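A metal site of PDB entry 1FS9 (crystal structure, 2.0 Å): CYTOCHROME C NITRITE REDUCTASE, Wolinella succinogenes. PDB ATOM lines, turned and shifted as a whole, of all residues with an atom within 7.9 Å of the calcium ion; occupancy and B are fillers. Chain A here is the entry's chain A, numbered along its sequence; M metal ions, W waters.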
ATOM      1  N   TYR A  90     -22.552 -37.787 -10.741  1.00  0.00           N
ATOM      2  CA  TYR A  90     -23.142 -37.640 -12.072  1.00  0.00           C
ATOM      3  C   TYR A  90     -22.790 -38.893 -12.896  1.00  0.00           C
ATOM      4  O   TYR A  90     -21.755 -39.517 -12.670  1.00  0.00           O
ATOM      5  CB  TYR A  90     -22.567 -36.369 -12.720  1.00  0.00           C
ATOM      6  CG  TYR A  90     -23.377 -35.783 -13.870  1.00  0.00           C
ATOM      7  CD1 TYR A  90     -24.691 -35.364 -13.687  1.00  0.00           C
ATOM      8  CD2 TYR A  90     -22.801 -35.606 -15.130  1.00  0.00           C
ATOM      9  CE1 TYR A  90     -25.420 -34.785 -14.734  1.00  0.00           C
ATOM     10  CE2 TYR A  90     -23.518 -35.044 -16.177  1.00  0.00           C
ATOM     11  CZ  TYR A  90     -24.828 -34.634 -15.974  1.00  0.00           C
ATOM     12  OH  TYR A  90     -25.525 -34.082 -17.031  1.00  0.00           O
ATOM     13  N   VAL A 216     -22.781 -29.672 -30.237  1.00  0.00           N
ATOM     14  CA  VAL A 216     -22.930 -28.427 -29.474  1.00  0.00           C
ATOM     15  C   VAL A 216     -23.224 -28.745 -28.009  1.00  0.00           C
ATOM     16  O   VAL A 216     -23.594 -29.873 -27.676  1.00  0.00           O
ATOM     17  CB  VAL A 216     -24.107 -27.591 -30.018  1.00  0.00           C
ATOM     18  CG1 VAL A 216     -23.814 -27.131 -31.447  1.00  0.00           C
ATOM     19  CG2 VAL A 216     -25.388 -28.421 -29.960  1.00  0.00           C
ATOM     20  N   GLU A 217     -23.064 -27.740 -27.154  1.00  0.00           N
ATOM     21  CA  GLU A 217     -23.342 -27.878 -25.729  1.00  0.00           C
ATOM     22  C   GLU A 217     -24.854 -27.685 -25.565  1.00  0.00           C
ATOM     23  O   GLU A 217     -25.490 -26.966 -26.351  1.00  0.00           O
ATOM     24  CB  GLU A 217     -22.555 -26.814 -24.945  1.00  0.00           C
ATOM     25  CG  GLU A 217     -23.239 -26.210 -23.715  1.00  0.00           C
ATOM     26  CD  GLU A 217     -23.522 -27.211 -22.600  1.00  0.00           C
ATOM     27  OE1 GLU A 217     -23.009 -28.358 -22.651  1.00  0.00           O
ATOM     28  OE2 GLU A 217     -24.250 -26.834 -21.662  1.00  0.00           O
ATOM     29  N   TYR A 218     -25.436 -28.330 -24.568  1.00  0.00           N
ATOM     30  CA  TYR A 218     -26.875 -28.234 -24.355  1.00  0.00           C
ATOM     31  C   TYR A 218     -27.245 -28.614 -22.925  1.00  0.00           C
ATOM     32  O   TYR A 218     -26.405 -29.077 -22.149  1.00  0.00           O
ATOM     33  CB  TYR A 218     -27.609 -29.199 -25.282  1.00  0.00           C
ATOM     34  CG  TYR A 218     -27.446 -30.636 -24.820  1.00  0.00           C
ATOM     35  CD1 TYR A 218     -26.268 -31.350 -25.063  1.00  0.00           C
ATOM     36  CD2 TYR A 218     -28.423 -31.228 -24.018  1.00  0.00           C
ATOM     37  CE1 TYR A 218     -26.068 -32.620 -24.501  1.00  0.00           C
ATOM     38  CE2 TYR A 218     -28.228 -32.490 -23.446  1.00  0.00           C
ATOM     39  CZ  TYR A 218     -27.051 -33.168 -23.687  1.00  0.00           C
ATOM     40  OH  TYR A 218     -26.857 -34.395 -23.084  1.00  0.00           O
ATOM     41  N   TYR A 219     -28.519 -28.434 -22.591  1.00  0.00           N
ATOM     42  CA  TYR A 219     -29.050 -28.846 -21.300  1.00  0.00           C
ATOM     43  C   TYR A 219     -30.502 -29.244 -21.521  1.00  0.00           C
ATOM     44  O   TYR A 219     -31.079 -28.913 -22.553  1.00  0.00           O
ATOM     45  CB  TYR A 219     -28.946 -27.725 -20.252  1.00  0.00           C
ATOM     46  CG  TYR A 219     -29.958 -26.608 -20.344  1.00  0.00           C
ATOM     47  CD1 TYR A 219     -29.779 -25.548 -21.230  1.00  0.00           C
ATOM     48  CD2 TYR A 219     -31.087 -26.592 -19.520  1.00  0.00           C
ATOM     49  CE1 TYR A 219     -30.696 -24.488 -21.281  1.00  0.00           C
ATOM     50  CE2 TYR A 219     -32.000 -25.541 -19.551  1.00  0.00           C
ATOM     51  CZ  TYR A 219     -31.793 -24.487 -20.436  1.00  0.00           C
ATOM     52  OH  TYR A 219     -32.678 -23.442 -20.456  1.00  0.00           O
ATOM     53  N   PHE A 220     -31.074 -29.989 -20.578  1.00  0.00           N
ATOM     54  CA  PHE A 220     -32.463 -30.419 -20.707  1.00  0.00           C
ATOM     55  C   PHE A 220     -33.345 -29.470 -19.910  1.00  0.00           C
ATOM     56  O   PHE A 220     -33.174 -29.317 -18.703  1.00  0.00           O
ATOM     57  CB  PHE A 220     -32.662 -31.846 -20.160  1.00  0.00           C
ATOM     58  CG  PHE A 220     -31.918 -32.899 -20.928  1.00  0.00           C
ATOM     59  CD1 PHE A 220     -31.800 -32.833 -22.313  1.00  0.00           C
ATOM     60  CD2 PHE A 220     -31.383 -33.996 -20.264  1.00  0.00           C
ATOM     61  CE1 PHE A 220     -31.150 -33.841 -23.033  1.00  0.00           C
ATOM     62  CE2 PHE A 220     -30.735 -35.019 -20.975  1.00  0.00           C
ATOM     63  CZ  PHE A 220     -30.615 -34.938 -22.359  1.00  0.00           C
ATOM     64  N   THR A 239     -32.039 -28.054 -25.099  1.00  0.00           N
ATOM     65  CA  THR A 239     -31.986 -26.610 -25.301  1.00  0.00           C
ATOM     66  C   THR A 239     -30.547 -26.144 -25.358  1.00  0.00           C
ATOM     67  O   THR A 239     -29.707 -26.572 -24.570  1.00  0.00           O
ATOM     68  CB  THR A 239     -32.687 -25.883 -24.136  1.00  0.00           C
ATOM     69  OG1 THR A 239     -34.019 -26.412 -23.977  1.00  0.00           O
ATOM     70  CG2 THR A 239     -32.777 -24.377 -24.401  1.00  0.00           C
ATOM     71  N   PRO A 241     -27.966 -23.394 -24.610  1.00  0.00           N
ATOM     72  CA  PRO A 241     -27.808 -22.247 -23.709  1.00  0.00           C
ATOM     73  C   PRO A 241     -27.154 -21.055 -24.397  1.00  0.00           C
ATOM     74  O   PRO A 241     -26.172 -20.506 -23.899  1.00  0.00           O
ATOM     75  CB  PRO A 241     -26.927 -22.809 -22.605  1.00  0.00           C
ATOM     76  CG  PRO A 241     -25.970 -23.672 -23.405  1.00  0.00           C
ATOM     77  CD  PRO A 241     -26.907 -24.399 -24.370  1.00  0.00           C
ATOM     78  N   MET A 251     -22.542 -18.357 -21.690  1.00  0.00           N
ATOM     79  CA  MET A 251     -23.314 -19.538 -21.307  1.00  0.00           C
ATOM     80  C   MET A 251     -23.318 -19.628 -19.778  1.00  0.00           C
ATOM     81  O   MET A 251     -24.328 -19.985 -19.177  1.00  0.00           O
ATOM     82  CB  MET A 251     -22.705 -20.804 -21.910  1.00  0.00           C
ATOM     83  CG  MET A 251     -22.927 -20.938 -23.399  1.00  0.00           C
ATOM     84  SD  MET A 251     -22.362 -22.534 -24.029  1.00  0.00           S
ATOM     85  CE  MET A 251     -21.472 -22.048 -25.471  1.00  0.00           C
ATOM     86  N   TYR A 255     -26.599 -19.822 -17.413  1.00  0.00           N
ATOM     87  CA  TYR A 255     -26.922 -20.823 -16.411  1.00  0.00           C
ATOM     88  C   TYR A 255     -27.075 -20.240 -15.008  1.00  0.00           C
ATOM     89  O   TYR A 255     -27.933 -20.680 -14.244  1.00  0.00           O
ATOM     90  CB  TYR A 255     -25.861 -21.930 -16.416  1.00  0.00           C
ATOM     91  CG  TYR A 255     -25.974 -22.899 -17.578  1.00  0.00           C
ATOM     92  CD1 TYR A 255     -27.157 -23.610 -17.792  1.00  0.00           C
ATOM     93  CD2 TYR A 255     -24.907 -23.123 -18.444  1.00  0.00           C
ATOM     94  CE1 TYR A 255     -27.265 -24.529 -18.830  1.00  0.00           C
ATOM     95  CE2 TYR A 255     -25.008 -24.049 -19.503  1.00  0.00           C
ATOM     96  CZ  TYR A 255     -26.196 -24.740 -19.686  1.00  0.00           C
ATOM     97  OH  TYR A 255     -26.321 -25.671 -20.696  1.00  0.00           O
ATOM     98  N   PHE A 260     -29.497 -22.650 -12.638  1.00  0.00           N
ATOM     99  CA  PHE A 260     -29.513 -24.022 -13.122  1.00  0.00           C
ATOM    100  C   PHE A 260     -28.326 -24.850 -12.618  1.00  0.00           C
ATOM    101  O   PHE A 260     -27.244 -24.315 -12.377  1.00  0.00           O
ATOM    102  CB  PHE A 260     -29.502 -24.048 -14.656  1.00  0.00           C
ATOM    103  CG  PHE A 260     -29.666 -25.421 -15.237  1.00  0.00           C
ATOM    104  CD1 PHE A 260     -30.931 -26.009 -15.299  1.00  0.00           C
ATOM    105  CD2 PHE A 260     -28.563 -26.145 -15.684  1.00  0.00           C
ATOM    106  CE1 PHE A 260     -31.087 -27.294 -15.805  1.00  0.00           C
ATOM    107  CE2 PHE A 260     -28.714 -27.438 -16.181  1.00  0.00           C
ATOM    108  CZ  PHE A 260     -29.976 -28.012 -16.241  1.00  0.00           C
ATOM    109  N   ASP A 262     -26.820 -29.075 -13.259  1.00  0.00           N
ATOM    110  CA  ASP A 262     -27.035 -30.385 -13.859  1.00  0.00           C
ATOM    111  C   ASP A 262     -27.071 -31.449 -12.768  1.00  0.00           C
ATOM    112  O   ASP A 262     -27.736 -32.478 -12.904  1.00  0.00           O
ATOM    113  CB  ASP A 262     -25.929 -30.689 -14.878  1.00  0.00           C
ATOM    114  CG  ASP A 262     -26.124 -29.943 -16.185  1.00  0.00           C
ATOM    115  OD1 ASP A 262     -27.096 -30.264 -16.913  1.00  0.00           O
ATOM    116  OD2 ASP A 262     -25.329 -29.024 -16.489  1.00  0.00           O
ATOM    117  N   LEU A 273     -22.383 -27.660 -13.264  1.00  0.00           N
ATOM    118  CA  LEU A 273     -22.775 -27.476 -14.655  1.00  0.00           C
ATOM    119  C   LEU A 273     -21.926 -28.447 -15.475  1.00  0.00           C
ATOM    120  O   LEU A 273     -20.701 -28.499 -15.314  1.00  0.00           O
ATOM    121  CB  LEU A 273     -22.483 -26.037 -15.107  1.00  0.00           C
ATOM    122  CG  LEU A 273     -23.336 -24.908 -14.531  1.00  0.00           C
ATOM    123  CD1 LEU A 273     -22.838 -23.571 -15.059  1.00  0.00           C
ATOM    124  CD2 LEU A 273     -24.795 -25.127 -14.944  1.00  0.00           C
ATOM    125  N   LYS A 274     -22.565 -29.217 -16.339  1.00  0.00           N
ATOM    126  CA  LYS A 274     -21.840 -30.161 -17.193  1.00  0.00           C
ATOM    127  C   LYS A 274     -21.728 -29.630 -18.606  1.00  0.00           C
ATOM    128  O   LYS A 274     -22.717 -29.232 -19.212  1.00  0.00           O
ATOM    129  CB  LYS A 274     -22.551 -31.511 -17.235  1.00  0.00           C
ATOM    130  CG  LYS A 274     -21.805 -32.562 -18.063  1.00  0.00           C
ATOM    131  CD  LYS A 274     -20.577 -33.079 -17.323  1.00  0.00           C
ATOM    132  CE  LYS A 274     -19.734 -34.016 -18.201  1.00  0.00           C
ATOM    133  NZ  LYS A 274     -18.880 -33.274 -19.183  1.00  0.00           N
ATOM    134  N   ALA A 275     -20.519 -29.633 -19.146  1.00  0.00           N
ATOM    135  CA  ALA A 275     -20.310 -29.181 -20.519  1.00  0.00           C
ATOM    136  C   ALA A 275     -20.300 -30.421 -21.397  1.00  0.00           C
ATOM    137  O   ALA A 275     -19.701 -31.434 -21.037  1.00  0.00           O
ATOM    138  CB  ALA A 275     -18.975 -28.459 -20.649  1.00  0.00           C
ATOM    139  N   GLN A 276     -20.984 -30.352 -22.535  1.00  0.00           N
ATOM    140  CA  GLN A 276     -20.985 -31.478 -23.459  1.00  0.00           C
ATOM    141  C   GLN A 276     -20.578 -31.050 -24.855  1.00  0.00           C
ATOM    142  O   GLN A 276     -21.215 -30.203 -25.474  1.00  0.00           O
ATOM    143  CB  GLN A 276     -22.349 -32.168 -23.539  1.00  0.00           C
ATOM    144  CG  GLN A 276     -22.691 -33.053 -22.352  1.00  0.00           C
ATOM    145  CD  GLN A 276     -23.657 -32.391 -21.401  1.00  0.00           C
ATOM    146  OE1 GLN A 276     -23.793 -31.172 -21.401  1.00  0.00           O
ATOM    147  NE2 GLN A 276     -24.338 -33.195 -20.586  1.00  0.00           N
ATOM    148  N   HIS A 277     -19.481 -31.634 -25.335  1.00  0.00           N
ATOM    149  CA  HIS A 277     -18.962 -31.397 -26.675  1.00  0.00           C
ATOM    150  C   HIS A 277     -19.416 -30.113 -27.367  1.00  0.00           C
ATOM    151  O   HIS A 277     -20.214 -30.148 -28.304  1.00  0.00           O
ATOM    152  CB  HIS A 277     -19.355 -32.593 -27.538  1.00  0.00           C
ATOM    153  CG  HIS A 277     -20.751 -33.069 -27.320  1.00  0.00           C
ATOM    154  ND1 HIS A 277     -21.858 -32.264 -27.561  1.00  0.00           N
ATOM    155  CD2 HIS A 277     -21.234 -34.228 -26.802  1.00  0.00           C
ATOM    156  CE1 HIS A 277     -22.954 -32.916 -27.207  1.00  0.00           C
ATOM    157  NE2 HIS A 277     -22.605 -34.109 -26.746  1.00  0.00           N
ATOM    158  N   TRP A 391     -16.907 -25.488 -14.932  1.00  0.00           N
ATOM    159  CA  TRP A 391     -17.680 -25.189 -16.124  1.00  0.00           C
ATOM    160  C   TRP A 391     -16.733 -24.720 -17.214  1.00  0.00           C
ATOM    161  O   TRP A 391     -16.831 -25.150 -18.360  1.00  0.00           O
ATOM    162  CB  TRP A 391     -18.716 -24.093 -15.848  1.00  0.00           C
ATOM    163  CG  TRP A 391     -19.303 -23.525 -17.099  1.00  0.00           C
ATOM    164  CD1 TRP A 391     -19.146 -22.259 -17.586  1.00  0.00           C
ATOM    165  CD2 TRP A 391     -20.112 -24.227 -18.068  1.00  0.00           C
ATOM    166  NE1 TRP A 391     -19.808 -22.126 -18.780  1.00  0.00           N
ATOM    167  CE2 TRP A 391     -20.407 -23.324 -19.102  1.00  0.00           C
ATOM    168  CE3 TRP A 391     -20.606 -25.539 -18.150  1.00  0.00           C
ATOM    169  CZ2 TRP A 391     -21.185 -23.678 -20.213  1.00  0.00           C
ATOM    170  CZ3 TRP A 391     -21.384 -25.894 -19.252  1.00  0.00           C
ATOM    171  CH2 TRP A 391     -21.657 -24.953 -20.272  1.00  0.00           C
ATOM    172  N   ASP A 394     -14.274 -27.654 -18.255  1.00  0.00           N
ATOM    173  CA  ASP A 394     -14.998 -28.713 -18.956  1.00  0.00           C
ATOM    174  C   ASP A 394     -15.331 -28.237 -20.362  1.00  0.00           C
ATOM    175  O   ASP A 394     -15.200 -28.998 -21.333  1.00  0.00           O
ATOM    176  CB  ASP A 394     -16.262 -29.087 -18.186  1.00  0.00           C
ATOM    177  CG  ASP A 394     -16.783 -30.473 -18.533  1.00  0.00           C
ATOM    178  OD1 ASP A 394     -16.115 -31.192 -19.319  1.00  0.00           O
ATOM    179  OD2 ASP A 394     -17.853 -30.857 -18.015  1.00  0.00           O
ATOM    180  N   MET A 395     -15.767 -26.988 -20.483  1.00  0.00           N
ATOM    181  CA  MET A 395     -16.093 -26.424 -21.804  1.00  0.00           C
ATOM    182  C   MET A 395     -14.853 -26.437 -22.683  1.00  0.00           C
ATOM    183  O   MET A 395     -14.951 -26.589 -23.907  1.00  0.00           O
ATOM    184  CB  MET A 395     -16.600 -24.986 -21.680  1.00  0.00           C
ATOM    185  CG  MET A 395     -18.073 -24.867 -21.367  1.00  0.00           C
ATOM    186  SD  MET A 395     -19.079 -25.464 -22.750  1.00  0.00           S
ATOM    187  CE  MET A 395     -18.956 -24.077 -23.863  1.00  0.00           C
HETATM  188 CA    CA M   1     -24.513 -29.009 -20.682  1.00  0.00          CA
HETATM  189  O   HOH W   1     -25.498 -27.714 -18.831  1.00  0.00           O
HETATM  190  O   HOH W   2     -26.050 -30.607 -19.378  1.00  0.00           O
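NZ of Lys 274 lies within salt-bridge range of OD2 of Asp 394 (2.9 Å). The backbone carbonyl oxygen (O) of Tyr 255 lies within hydrogen-bond range of the backbone NH (N) of Phe 260 (3.0 Å). OE2 of Glu 217 lies close to OH of Tyr 255, at 2.6 Å. The side-chain carboxylate of Asp 262 lies within hydrogen-bond range of the backbone NH of Lys 274, 2.8 Å away.
Water W1 lies within hydrogen-bond range of OD2 of Asp 262 (2.7 Å) and OH of Tyr 255 (2.9 Å). Water W2 lies within hydrogen-bond range of the side-chain carboxylate of Asp 262 and the side-chain amide nitrogen of Gln 276.
The backbone carbonyl oxygen (O) of Lys 274 binds the calcium ion. The side-chain amide oxygen (OE1) of Gln 276 binds the calcium ion (2.4 Å). O of Tyr 218 is bound to the calcium ion, 2.4 Å away. OE2 of Glu 217 is bound to the calcium ion. The calcium ion is bound by water W1 (2.5 Å). OE1 of Glu 217 is bound to the calcium ion (2.6 Å). The calcium ion is bound by water W2 (2.6 Å).
Tyr 255 touches the calcium ion. Of the 20 residues printed, 5 come within 4 Å of the calcium ion. The nearest printed residue that does not touch the calcium ion is Ala 275 (4.2 Å).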
